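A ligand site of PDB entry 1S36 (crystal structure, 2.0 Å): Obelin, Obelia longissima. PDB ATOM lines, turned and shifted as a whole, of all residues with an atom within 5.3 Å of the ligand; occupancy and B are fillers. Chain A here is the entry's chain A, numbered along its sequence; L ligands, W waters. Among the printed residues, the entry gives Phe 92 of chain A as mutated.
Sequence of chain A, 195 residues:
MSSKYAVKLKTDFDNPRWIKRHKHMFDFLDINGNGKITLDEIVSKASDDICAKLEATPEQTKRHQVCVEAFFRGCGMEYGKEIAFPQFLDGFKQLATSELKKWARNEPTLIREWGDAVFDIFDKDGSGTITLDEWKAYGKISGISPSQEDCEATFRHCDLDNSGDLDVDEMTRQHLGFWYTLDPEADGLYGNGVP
NE2 of His 64 is in hydrogen-bond range of NE1 of Trp 114 (3.2 Å).
The backbone carbonyl oxygen (O) of Met 171 sits at hydrogen-bond distance from a ring nitrogen (ND1) of His 175 (2.8 Å).
The backbone carbonyl oxygen (O) of Lys 45 is in hydrogen-bond range of the backbone NH (N) of Ile 50, 3.0 Å away.
NE2 of His 175 lies within hydrogen-bond range of OH of Tyr 190 (2.5 Å).
A ring nitrogen (NE2) of His 64 sits at hydrogen-bond distance from the side-chain hydroxyl (OH) of Tyr 138.
The backbone carbonyl oxygen (O) of Trp 179 is in hydrogen-bond range of a ring nitrogen (NE2) of His 22 (2.9 Å).
The side-chain hydroxyl (OG) of Ser 142 sits close to the backbone NH (N) of Ile 144 (3.3 Å).
OG of Ser 142 is in hydrogen-bond range of O of Tyr 138 (2.8 Å).
A ring nitrogen (ND1) of His 175 lies within hydrogen-bond range of an oxygen (O2) of the ligand, 3.4 Å away.
A ring nitrogen (ND1) of His 22 is in hydrogen-bond range of an oxygen (O3) of the ligand (2.8 Å).
Water W2 lies within hydrogen-bond range of an oxygen (O2) of the ligand (2.6 Å), the backbone carbonyl oxygen (O) of Ile 111 (2.7 Å) and the side-chain hydroxyl (OG1) of Thr 172 (2.7 Å).
Water W3 lies within hydrogen-bond range of O1 of the ligand and OH of Tyr 190.
Water W1 bridges the indole nitrogen (NE1) of Trp 179 (2.8 Å) and a nitrogen (N3) of the ligand (3.0 Å).
Residues that only touch the ligand: Trp 114 (3.2 Å), Tyr 138 (3.2 Å), Phe 88 (3.3 Å), Met 171 (3.3 Å), Met 25 (3.4 Å), Phe 92 (3.5 Å), Trp 179 (3.5 Å), Gly 115 (3.7 Å), Ile 111 (3.7 Å), Ile 50 (3.7 Å), Leu 29 (3.7 Å), Ile 42 (3.8 Å), Phe 72 (3.9 Å), Ile 144 (3.9 Å), Phe 71 (3.9 Å), Val 118 (3.9 Å) and Trp 135 (3.9 Å).
Hydrophobic or aromatic side chains within 4 Å of the ligand: His 22, Met 25, Leu 29, Ile 42, Ile 50, Phe 71, Phe 72, Phe 88, Phe 92, Ile 111, Trp 114, Val 118, Trp 135, Tyr 138, Ile 144, Met 171, His 175 and Trp 179.
Within 4 Å of the ligand: His 22, Met 25, Leu 29, Ile 42, Ile 50, Phe 71, Phe 72, Phe 88, Phe 92, Ile 111, Trp 114, Gly 115, Val 118, Trp 135, Tyr 138, Ile 144, Met 171, His 175 and Trp 179.
The nearest printed residue that does not touch the ligand is Ala 46 (4.1 Å).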
ATOM      1  N   HIS A  22      -7.286  -4.422   2.789  1.00  0.00           N
ATOM      2  CA  HIS A  22      -6.322  -4.262   3.899  1.00  0.00           C
ATOM      3  C   HIS A  22      -5.058  -5.068   3.768  1.00  0.00           C
ATOM      4  O   HIS A  22      -3.984  -4.620   4.180  1.00  0.00           O
ATOM      5  CB  HIS A  22      -7.050  -4.376   5.245  1.00  0.00           C
ATOM      6  CG  HIS A  22      -7.971  -3.224   5.465  1.00  0.00           C
ATOM      7  ND1 HIS A  22      -7.520  -1.932   5.666  1.00  0.00           N
ATOM      8  CD2 HIS A  22      -9.321  -3.129   5.375  1.00  0.00           C
ATOM      9  CE1 HIS A  22      -8.543  -1.112   5.745  1.00  0.00           C
ATOM     10  NE2 HIS A  22      -9.650  -1.822   5.588  1.00  0.00           N
ATOM     11  N   MET A  25      -2.811  -3.023   1.624  1.00  0.00           N
ATOM     12  CA  MET A  25      -2.176  -1.978   2.418  1.00  0.00           C
ATOM     13  C   MET A  25      -1.123  -2.548   3.362  1.00  0.00           C
ATOM     14  O   MET A  25      -0.083  -1.914   3.578  1.00  0.00           O
ATOM     15  CB  MET A  25      -3.238  -1.196   3.209  1.00  0.00           C
ATOM     16  CG  MET A  25      -4.194  -0.337   2.340  1.00  0.00           C
ATOM     17  SD  MET A  25      -3.273   0.693   1.174  1.00  0.00           S
ATOM     18  CE  MET A  25      -2.421   1.878   2.302  1.00  0.00           C
ATOM     19  N   PHE A  26      -1.412  -3.718   3.941  1.00  0.00           N
ATOM     20  CA  PHE A  26      -0.470  -4.350   4.860  1.00  0.00           C
ATOM     21  C   PHE A  26       0.809  -4.772   4.135  1.00  0.00           C
ATOM     22  O   PHE A  26       1.924  -4.542   4.618  1.00  0.00           O
ATOM     23  CB  PHE A  26      -1.123  -5.544   5.557  1.00  0.00           C
ATOM     24  CG  PHE A  26      -0.212  -6.270   6.543  1.00  0.00           C
ATOM     25  CD1 PHE A  26      -0.335  -6.052   7.909  1.00  0.00           C
ATOM     26  CD2 PHE A  26       0.728  -7.203   6.088  1.00  0.00           C
ATOM     27  CE1 PHE A  26       0.482  -6.722   8.813  1.00  0.00           C
ATOM     28  CE2 PHE A  26       1.575  -7.896   6.995  1.00  0.00           C
ATOM     29  CZ  PHE A  26       1.439  -7.660   8.360  1.00  0.00           C
ATOM     30  N   PHE A  28       1.936  -3.418   1.489  1.00  0.00           N
ATOM     31  CA  PHE A  28       2.597  -2.160   1.121  1.00  0.00           C
ATOM     32  C   PHE A  28       3.474  -1.643   2.289  1.00  0.00           C
ATOM     33  O   PHE A  28       4.598  -1.168   2.056  1.00  0.00           O
ATOM     34  CB  PHE A  28       1.538  -1.146   0.655  1.00  0.00           C
ATOM     35  CG  PHE A  28       1.915   0.311   0.817  1.00  0.00           C
ATOM     36  CD1 PHE A  28       2.936   0.891   0.073  1.00  0.00           C
ATOM     37  CD2 PHE A  28       1.176   1.120   1.699  1.00  0.00           C
ATOM     38  CE1 PHE A  28       3.250   2.249   0.219  1.00  0.00           C
ATOM     39  CE2 PHE A  28       1.488   2.486   1.840  1.00  0.00           C
ATOM     40  CZ  PHE A  28       2.515   3.050   1.105  1.00  0.00           C
ATOM     41  N   LEU A  29       2.976  -1.762   3.506  1.00  0.00           N
ATOM     42  CA  LEU A  29       3.755  -1.298   4.659  1.00  0.00           C
ATOM     43  C   LEU A  29       4.780  -2.312   5.148  1.00  0.00           C
ATOM     44  O   LEU A  29       5.679  -1.967   5.936  1.00  0.00           O
ATOM     45  CB  LEU A  29       2.839  -0.872   5.790  1.00  0.00           C
ATOM     46  CG  LEU A  29       1.912   0.295   5.480  1.00  0.00           C
ATOM     47  CD1 LEU A  29       0.851   0.333   6.535  1.00  0.00           C
ATOM     48  CD2 LEU A  29       2.674   1.597   5.474  1.00  0.00           C
ATOM     49  N   ILE A  42       6.696   2.304  10.154  1.00  0.00           N
ATOM     50  CA  ILE A  42       5.605   3.153   9.656  1.00  0.00           C
ATOM     51  C   ILE A  42       5.791   4.659   9.989  1.00  0.00           C
ATOM     52  O   ILE A  42       5.716   5.507   9.091  1.00  0.00           O
ATOM     53  CB  ILE A  42       4.244   2.637  10.196  1.00  0.00           C
ATOM     54  CG1 ILE A  42       3.880   1.348   9.471  1.00  0.00           C
ATOM     55  CG2 ILE A  42       3.124   3.681  10.013  1.00  0.00           C
ATOM     56  CD1 ILE A  42       2.655   0.651  10.043  1.00  0.00           C
ATOM     57  N   LYS A  45       8.697   6.148   8.172  1.00  0.00           N
ATOM     58  CA  LYS A  45       8.170   6.454   6.823  1.00  0.00           C
ATOM     59  C   LYS A  45       7.358   7.746   6.767  1.00  0.00           C
ATOM     60  O   LYS A  45       7.530   8.557   5.856  1.00  0.00           O
ATOM     61  CB  LYS A  45       7.332   5.275   6.286  1.00  0.00           C
ATOM     62  CG  LYS A  45       6.379   5.605   5.127  1.00  0.00           C
ATOM     63  CD  LYS A  45       5.543   4.374   4.724  1.00  0.00           C
ATOM     64  CE  LYS A  45       4.923   4.560   3.360  1.00  0.00           C
ATOM     65  NZ  LYS A  45       6.040   4.622   2.329  1.00  0.00           N
ATOM     66  N   ALA A  46       6.471   7.945   7.740  1.00  0.00           N
ATOM     67  CA  ALA A  46       5.692   9.177   7.805  1.00  0.00           C
ATOM     68  C   ALA A  46       6.576  10.420   7.977  1.00  0.00           C
ATOM     69  O   ALA A  46       6.396  11.444   7.284  1.00  0.00           O
ATOM     70  CB  ALA A  46       4.686   9.083   8.931  1.00  0.00           C
ATOM     71  N   ILE A  50       8.269  10.838   4.086  1.00  0.00           N
ATOM     72  CA  ILE A  50       7.175  11.637   3.510  1.00  0.00           C
ATOM     73  C   ILE A  50       7.268  13.119   3.885  1.00  0.00           C
ATOM     74  O   ILE A  50       7.267  13.975   2.999  1.00  0.00           O
ATOM     75  CB  ILE A  50       5.768  11.043   3.868  1.00  0.00           C
ATOM     76  CG1 ILE A  50       5.550   9.729   3.132  1.00  0.00           C
ATOM     77  CG2 ILE A  50       4.622  11.993   3.455  1.00  0.00           C
ATOM     78  CD1 ILE A  50       4.581   8.763   3.831  1.00  0.00           C
ATOM     79  N   HIS A  64       1.500  15.568  11.854  1.00  0.00           N
ATOM     80  CA  HIS A  64       1.349  14.382  10.996  1.00  0.00           C
ATOM     81  C   HIS A  64       1.796  13.094  11.744  1.00  0.00           C
ATOM     82  O   HIS A  64       1.130  12.040  11.665  1.00  0.00           O
ATOM     83  CB  HIS A  64       2.106  14.589   9.677  1.00  0.00           C
ATOM     84  CG  HIS A  64       1.901  13.500   8.671  1.00  0.00           C
ATOM     85  ND1 HIS A  64       2.714  12.383   8.606  1.00  0.00           N
ATOM     86  CD2 HIS A  64       0.985  13.358   7.687  1.00  0.00           C
ATOM     87  CE1 HIS A  64       2.312  11.606   7.617  1.00  0.00           C
ATOM     88  NE2 HIS A  64       1.270  12.169   7.043  1.00  0.00           N
ATOM     89  N   VAL A  68      -0.506   9.653  12.613  1.00  0.00           N
ATOM     90  CA  VAL A  68      -0.074   8.316  12.212  1.00  0.00           C
ATOM     91  C   VAL A  68       0.005   7.394  13.441  1.00  0.00           C
ATOM     92  O   VAL A  68      -0.531   6.281  13.438  1.00  0.00           O
ATOM     93  CB  VAL A  68       1.291   8.395  11.478  1.00  0.00           C
ATOM     94  CG1 VAL A  68       1.842   6.998  11.184  1.00  0.00           C
ATOM     95  CG2 VAL A  68       1.152   9.185  10.185  1.00  0.00           C
ATOM     96  N   PHE A  71      -3.496   6.480  14.728  1.00  0.00           N
ATOM     97  CA  PHE A  71      -4.206   5.595  13.812  1.00  0.00           C
ATOM     98  C   PHE A  71      -3.703   4.145  14.003  1.00  0.00           C
ATOM     99  O   PHE A  71      -4.488   3.214  14.248  1.00  0.00           O
ATOM    100  CB  PHE A  71      -3.977   6.122  12.378  1.00  0.00           C
ATOM    101  CG  PHE A  71      -4.706   5.380  11.286  1.00  0.00           C
ATOM    102  CD1 PHE A  71      -5.944   5.829  10.834  1.00  0.00           C
ATOM    103  CD2 PHE A  71      -4.112   4.281  10.656  1.00  0.00           C
ATOM    104  CE1 PHE A  71      -6.624   5.165   9.776  1.00  0.00           C
ATOM    105  CE2 PHE A  71      -4.760   3.607   9.602  1.00  0.00           C
ATOM    106  CZ  PHE A  71      -6.031   4.050   9.162  1.00  0.00           C
ATOM    107  N   PHE A  72      -2.394   3.951  13.960  1.00  0.00           N
ATOM    108  CA  PHE A  72      -1.880   2.593  14.092  1.00  0.00           C
ATOM    109  C   PHE A  72      -1.910   2.018  15.525  1.00  0.00           C
ATOM    110  O   PHE A  72      -2.109   0.822  15.711  1.00  0.00           O
ATOM    111  CB  PHE A  72      -0.559   2.468  13.376  1.00  0.00           C
ATOM    112  CG  PHE A  72      -0.688   2.625  11.911  1.00  0.00           C
ATOM    113  CD1 PHE A  72      -0.397   3.827  11.302  1.00  0.00           C
ATOM    114  CD2 PHE A  72      -1.173   1.559  11.136  1.00  0.00           C
ATOM    115  CE1 PHE A  72      -0.552   3.978   9.965  1.00  0.00           C
ATOM    116  CE2 PHE A  72      -1.332   1.690   9.785  1.00  0.00           C
ATOM    117  CZ  PHE A  72      -1.027   2.925   9.183  1.00  0.00           C
ATOM    118  N   PHE A  88      -3.357  -7.549  12.963  1.00  0.00           N
ATOM    119  CA  PHE A  88      -3.539  -6.175  12.450  1.00  0.00           C
ATOM    120  C   PHE A  88      -4.975  -5.979  11.976  1.00  0.00           C
ATOM    121  O   PHE A  88      -5.579  -4.910  12.229  1.00  0.00           O
ATOM    122  CB  PHE A  88      -2.556  -5.868  11.326  1.00  0.00           C
ATOM    123  CG  PHE A  88      -2.843  -4.553  10.614  1.00  0.00           C
ATOM    124  CD1 PHE A  88      -2.462  -3.341  11.188  1.00  0.00           C
ATOM    125  CD2 PHE A  88      -3.536  -4.541   9.402  1.00  0.00           C
ATOM    126  CE1 PHE A  88      -2.774  -2.117  10.549  1.00  0.00           C
ATOM    127  CE2 PHE A  88      -3.835  -3.335   8.764  1.00  0.00           C
ATOM    128  CZ  PHE A  88      -3.444  -2.133   9.335  1.00  0.00           C
ATOM    129  N   PHE A  92      -7.704  -3.423  13.106  1.00  0.00           N
ATOM    130  CA  PHE A  92      -8.282  -2.462  12.176  1.00  0.00           C
ATOM    131  C   PHE A  92      -9.799  -2.457  12.314  1.00  0.00           C
ATOM    132  O   PHE A  92     -10.414  -1.398  12.283  1.00  0.00           O
ATOM    133  CB  PHE A  92      -7.834  -2.710  10.732  1.00  0.00           C
ATOM    134  CG  PHE A  92      -7.917  -1.480   9.865  1.00  0.00           C
ATOM    135  CD1 PHE A  92      -6.806  -0.680   9.667  1.00  0.00           C
ATOM    136  CD2 PHE A  92      -9.144  -1.082   9.321  1.00  0.00           C
ATOM    137  CE1 PHE A  92      -6.903   0.513   8.904  1.00  0.00           C
ATOM    138  CE2 PHE A  92      -9.262   0.092   8.582  1.00  0.00           C
ATOM    139  CZ  PHE A  92      -8.131   0.888   8.362  1.00  0.00           C
ATOM    140  N   ILE A 111      -9.125   9.687  11.101  1.00  0.00           N
ATOM    141  CA  ILE A 111      -8.857   9.876   9.686  1.00  0.00           C
ATOM    142  C   ILE A 111      -9.105  11.340   9.263  1.00  0.00           C
ATOM    143  O   ILE A 111      -8.371  11.854   8.440  1.00  0.00           O
ATOM    144  CB  ILE A 111      -9.597   8.798   8.798  1.00  0.00           C
ATOM    145  CG1 ILE A 111      -9.027   8.728   7.373  1.00  0.00           C
ATOM    146  CG2 ILE A 111     -11.061   9.063   8.713  1.00  0.00           C
ATOM    147  CD1 ILE A 111      -7.593   8.357   7.281  1.00  0.00           C
ATOM    148  N   TRP A 114      -5.936  13.198  10.594  1.00  0.00           N
ATOM    149  CA  TRP A 114      -4.807  12.916   9.709  1.00  0.00           C
ATOM    150  C   TRP A 114      -4.934  13.735   8.394  1.00  0.00           C
ATOM    151  O   TRP A 114      -3.981  14.375   7.950  1.00  0.00           O
ATOM    152  CB  TRP A 114      -4.756  11.413   9.430  1.00  0.00           C
ATOM    153  CG  TRP A 114      -3.481  10.865   8.858  1.00  0.00           C
ATOM    154  CD1 TRP A 114      -2.356  11.566   8.441  1.00  0.00           C
ATOM    155  CD2 TRP A 114      -3.181   9.478   8.644  1.00  0.00           C
ATOM    156  NE1 TRP A 114      -1.398  10.678   7.995  1.00  0.00           N
ATOM    157  CE2 TRP A 114      -1.872   9.402   8.115  1.00  0.00           C
ATOM    158  CE3 TRP A 114      -3.888   8.290   8.877  1.00  0.00           C
ATOM    159  CZ2 TRP A 114      -1.261   8.177   7.795  1.00  0.00           C
ATOM    160  CZ3 TRP A 114      -3.289   7.077   8.543  1.00  0.00           C
ATOM    161  CH2 TRP A 114      -1.996   7.029   8.010  1.00  0.00           C
ATOM    162  N   GLY A 115      -6.112  13.749   7.788  1.00  0.00           N
ATOM    163  CA  GLY A 115      -6.349  14.610   6.641  1.00  0.00           C
ATOM    164  C   GLY A 115      -6.060  16.087   6.910  1.00  0.00           C
ATOM    165  O   GLY A 115      -5.468  16.758   6.082  1.00  0.00           O
ATOM    166  N   VAL A 118      -2.365  16.504   6.787  1.00  0.00           N
ATOM    167  CA  VAL A 118      -1.898  16.445   5.388  1.00  0.00           C
ATOM    168  C   VAL A 118      -2.186  17.777   4.714  1.00  0.00           C
ATOM    169  O   VAL A 118      -1.290  18.398   4.123  1.00  0.00           O
ATOM    170  CB  VAL A 118      -2.573  15.302   4.585  1.00  0.00           C
ATOM    171  CG1 VAL A 118      -2.262  15.402   3.071  1.00  0.00           C
ATOM    172  CG2 VAL A 118      -2.141  13.916   5.113  1.00  0.00           C
ATOM    173  N   TRP A 135      -1.847  16.389  -4.256  1.00  0.00           N
ATOM    174  CA  TRP A 135      -2.213  14.997  -4.019  1.00  0.00           C
ATOM    175  C   TRP A 135      -1.236  14.041  -4.698  1.00  0.00           C
ATOM    176  O   TRP A 135      -0.802  13.080  -4.081  1.00  0.00           O
ATOM    177  CB  TRP A 135      -3.629  14.742  -4.531  1.00  0.00           C
ATOM    178  CG  TRP A 135      -4.138  13.336  -4.342  1.00  0.00           C
ATOM    179  CD1 TRP A 135      -4.414  12.433  -5.318  1.00  0.00           C
ATOM    180  CD2 TRP A 135      -4.431  12.685  -3.101  1.00  0.00           C
ATOM    181  NE1 TRP A 135      -4.877  11.256  -4.776  1.00  0.00           N
ATOM    182  CE2 TRP A 135      -4.903  11.389  -3.417  1.00  0.00           C
ATOM    183  CE3 TRP A 135      -4.368  13.075  -1.753  1.00  0.00           C
ATOM    184  CZ2 TRP A 135      -5.296  10.461  -2.421  1.00  0.00           C
ATOM    185  CZ3 TRP A 135      -4.754  12.168  -0.766  1.00  0.00           C
ATOM    186  CH2 TRP A 135      -5.209  10.877  -1.108  1.00  0.00           C
ATOM    187  N   TYR A 138       1.875  13.669  -2.578  1.00  0.00           N
ATOM    188  CA  TYR A 138       1.683  12.745  -1.450  1.00  0.00           C
ATOM    189  C   TYR A 138       1.606  11.301  -1.952  1.00  0.00           C
ATOM    190  O   TYR A 138       2.292  10.428  -1.430  1.00  0.00           O
ATOM    191  CB  TYR A 138       0.459  13.120  -0.570  1.00  0.00           C
ATOM    192  CG  TYR A 138       0.502  12.513   0.840  1.00  0.00           C
ATOM    193  CD1 TYR A 138       0.864  13.281   1.958  1.00  0.00           C
ATOM    194  CD2 TYR A 138       0.157  11.162   1.050  1.00  0.00           C
ATOM    195  CE1 TYR A 138       0.891  12.728   3.248  1.00  0.00           C
ATOM    196  CE2 TYR A 138       0.183  10.587   2.343  1.00  0.00           C
ATOM    197  CZ  TYR A 138       0.557  11.377   3.427  1.00  0.00           C
ATOM    198  OH  TYR A 138       0.577  10.814   4.700  1.00  0.00           O
ATOM    199  N   SER A 142       4.506   9.069  -0.578  1.00  0.00           N
ATOM    200  CA  SER A 142       4.079   7.988   0.341  1.00  0.00           C
ATOM    201  C   SER A 142       4.094   6.601  -0.304  1.00  0.00           C
ATOM    202  O   SER A 142       4.071   5.594   0.402  1.00  0.00           O
ATOM    203  CB  SER A 142       2.679   8.263   0.892  1.00  0.00           C
ATOM    204  OG  SER A 142       1.683   7.994  -0.080  1.00  0.00           O
ATOM    205  N   ILE A 144       1.699   5.164  -1.774  1.00  0.00           N
ATOM    206  CA  ILE A 144       0.371   4.577  -1.826  1.00  0.00           C
ATOM    207  C   ILE A 144      -0.192   4.555  -3.256  1.00  0.00           C
ATOM    208  O   ILE A 144      -0.918   3.631  -3.630  1.00  0.00           O
ATOM    209  CB  ILE A 144      -0.603   5.300  -0.834  1.00  0.00           C
ATOM    210  CG1 ILE A 144      -1.869   4.465  -0.597  1.00  0.00           C
ATOM    211  CG2 ILE A 144      -0.952   6.701  -1.314  1.00  0.00           C
ATOM    212  CD1 ILE A 144      -2.816   5.040   0.456  1.00  0.00           C
ATOM    213  N   MET A 171     -12.527  14.400   1.155  1.00  0.00           N
ATOM    214  CA  MET A 171     -11.471  13.391   1.313  1.00  0.00           C
ATOM    215  C   MET A 171     -11.779  12.461   2.514  1.00  0.00           C
ATOM    216  O   MET A 171     -11.623  11.231   2.443  1.00  0.00           O
ATOM    217  CB  MET A 171     -10.108  14.077   1.451  1.00  0.00           C
ATOM    218  CG  MET A 171      -8.896  13.138   1.374  1.00  0.00           C
ATOM    219  SD  MET A 171      -7.363  14.128   1.542  1.00  0.00           S
ATOM    220  CE  MET A 171      -7.299  14.259   3.371  1.00  0.00           C
ATOM    221  N   THR A 172     -12.236  13.051   3.609  1.00  0.00           N
ATOM    222  CA  THR A 172     -12.624  12.299   4.804  1.00  0.00           C
ATOM    223  C   THR A 172     -13.752  11.287   4.562  1.00  0.00           C
ATOM    224  O   THR A 172     -13.624  10.107   4.914  1.00  0.00           O
ATOM    225  CB  THR A 172     -12.952  13.291   5.946  1.00  0.00           C
ATOM    226  OG1 THR A 172     -11.754  13.966   6.330  1.00  0.00           O
ATOM    227  CG2 THR A 172     -13.381  12.576   7.248  1.00  0.00           C
ATOM    228  N   HIS A 175     -12.611   8.381   2.401  1.00  0.00           N
ATOM    229  CA  HIS A 175     -11.711   7.441   3.066  1.00  0.00           C
ATOM    230  C   HIS A 175     -12.393   6.651   4.198  1.00  0.00           C
ATOM    231  O   HIS A 175     -12.038   5.487   4.442  1.00  0.00           O
ATOM    232  CB  HIS A 175     -10.426   8.146   3.499  1.00  0.00           C
ATOM    233  CG  HIS A 175      -9.487   8.417   2.353  1.00  0.00           C
ATOM    234  ND1 HIS A 175      -9.589   9.534   1.555  1.00  0.00           N
ATOM    235  CD2 HIS A 175      -8.456   7.698   1.868  1.00  0.00           C
ATOM    236  CE1 HIS A 175      -8.651   9.493   0.634  1.00  0.00           C
ATOM    237  NE2 HIS A 175      -7.952   8.383   0.791  1.00  0.00           N
ATOM    238  N   TRP A 179     -11.839   2.751   3.798  1.00  0.00           N
ATOM    239  CA  TRP A 179     -11.131   1.927   4.774  1.00  0.00           C
ATOM    240  C   TRP A 179     -12.101   1.195   5.699  1.00  0.00           C
ATOM    241  O   TRP A 179     -11.861   0.049   6.066  1.00  0.00           O
ATOM    242  CB  TRP A 179     -10.141   2.757   5.616  1.00  0.00           C
ATOM    243  CG  TRP A 179      -9.132   3.545   4.829  1.00  0.00           C
ATOM    244  CD1 TRP A 179      -8.836   4.869   4.990  1.00  0.00           C
ATOM    245  CD2 TRP A 179      -8.270   3.065   3.793  1.00  0.00           C
ATOM    246  NE1 TRP A 179      -7.846   5.231   4.099  1.00  0.00           N
ATOM    247  CE2 TRP A 179      -7.486   4.149   3.359  1.00  0.00           C
ATOM    248  CE3 TRP A 179      -8.081   1.811   3.180  1.00  0.00           C
ATOM    249  CZ2 TRP A 179      -6.525   4.032   2.333  1.00  0.00           C
ATOM    250  CZ3 TRP A 179      -7.131   1.687   2.173  1.00  0.00           C
ATOM    251  CH2 TRP A 179      -6.357   2.793   1.767  1.00  0.00           C
ATOM    252  N   TYR A 190      -8.838   5.061  -5.442  1.00  0.00           N
ATOM    253  CA  TYR A 190      -7.435   5.090  -5.816  1.00  0.00           C
ATOM    254  C   TYR A 190      -7.173   4.573  -7.228  1.00  0.00           C
ATOM    255  O   TYR A 190      -6.064   4.136  -7.517  1.00  0.00           O
ATOM    256  CB  TYR A 190      -6.597   4.310  -4.766  1.00  0.00           C
ATOM    257  CG  TYR A 190      -6.361   5.153  -3.543  1.00  0.00           C
ATOM    258  CD1 TYR A 190      -7.254   5.129  -2.474  1.00  0.00           C
ATOM    259  CD2 TYR A 190      -5.255   6.012  -3.464  1.00  0.00           C
ATOM    260  CE1 TYR A 190      -7.054   5.925  -1.347  1.00  0.00           C
ATOM    261  CE2 TYR A 190      -5.041   6.812  -2.339  1.00  0.00           C
ATOM    262  CZ  TYR A 190      -5.961   6.768  -1.292  1.00  0.00           C
ATOM    263  OH  TYR A 190      -5.775   7.555  -0.176  1.00  0.00           O
HETATM  264  O1  LIG L   1      -2.669   8.201   2.707  1.00  0.00           O
HETATM  265  C1  LIG L   1      -2.751   8.804   3.752  1.00  0.00           C
HETATM  266  C2  LIG L   1      -2.723  10.322   3.758  1.00  0.00           C
HETATM  267  C3  LIG L   1      -4.228  10.603   3.908  1.00  0.00           C
HETATM  268  C4  LIG L   1      -4.774  10.871   5.146  1.00  0.00           C
HETATM  269  C5  LIG L   1      -6.164  11.100   5.274  1.00  0.00           C
HETATM  270  C6  LIG L   1      -6.988  11.014   4.146  1.00  0.00           C
HETATM  271  O2  LIG L   1      -8.407  11.239   4.260  1.00  0.00           O
HETATM  272  C7  LIG L   1      -6.439  10.710   2.901  1.00  0.00           C
HETATM  273  C8  LIG L   1      -5.059  10.496   2.790  1.00  0.00           C
HETATM  274  N1  LIG L   1      -2.861   8.178   4.912  1.00  0.00           N
HETATM  275  C9  LIG L   1      -3.096   6.734   5.018  1.00  0.00           C
HETATM  276  C10 LIG L   1      -2.117   5.769   4.687  1.00  0.00           C
HETATM  277  C11 LIG L   1      -0.768   6.182   4.110  1.00  0.00           C
HETATM  278  C12 LIG L   1       0.352   6.146   5.132  1.00  0.00           C
HETATM  279  C13 LIG L   1       1.138   7.273   5.326  1.00  0.00           C
HETATM  280  C14 LIG L   1       2.189   7.257   6.268  1.00  0.00           C
HETATM  281  C15 LIG L   1       2.437   6.091   7.004  1.00  0.00           C
HETATM  282  C16 LIG L   1       1.654   4.950   6.801  1.00  0.00           C
HETATM  283  C17 LIG L   1       0.606   4.980   5.860  1.00  0.00           C
HETATM  284  N2  LIG L   1      -2.412   4.461   4.855  1.00  0.00           N
HETATM  285  C18 LIG L   1      -3.619   4.089   5.367  1.00  0.00           C
HETATM  286  C19 LIG L   1      -4.552   5.054   5.714  1.00  0.00           C
HETATM  287  N3  LIG L   1      -4.294   6.330   5.530  1.00  0.00           N
HETATM  288  C20 LIG L   1      -3.917   2.710   5.583  1.00  0.00           C
HETATM  289  C21 LIG L   1      -2.913   1.830   5.978  1.00  0.00           C
HETATM  290  C22 LIG L   1      -3.224   0.481   6.218  1.00  0.00           C
HETATM  291  C23 LIG L   1      -4.523   0.030   6.064  1.00  0.00           C
HETATM  292  O3  LIG L   1      -4.832  -1.339   6.284  1.00  0.00           O
HETATM  293  C24 LIG L   1      -5.531   0.919   5.665  1.00  0.00           C
HETATM  294  C25 LIG L   1      -5.237   2.263   5.450  1.00  0.00           C
HETATM  295  O   HOH W   1      -6.507   7.703   4.140  1.00  0.00           O
HETATM  296  O   HOH W   2      -9.274  12.839   6.129  1.00  0.00           O
HETATM  297  O   HOH W   3      -3.148   8.612   0.122  1.00  0.00           O
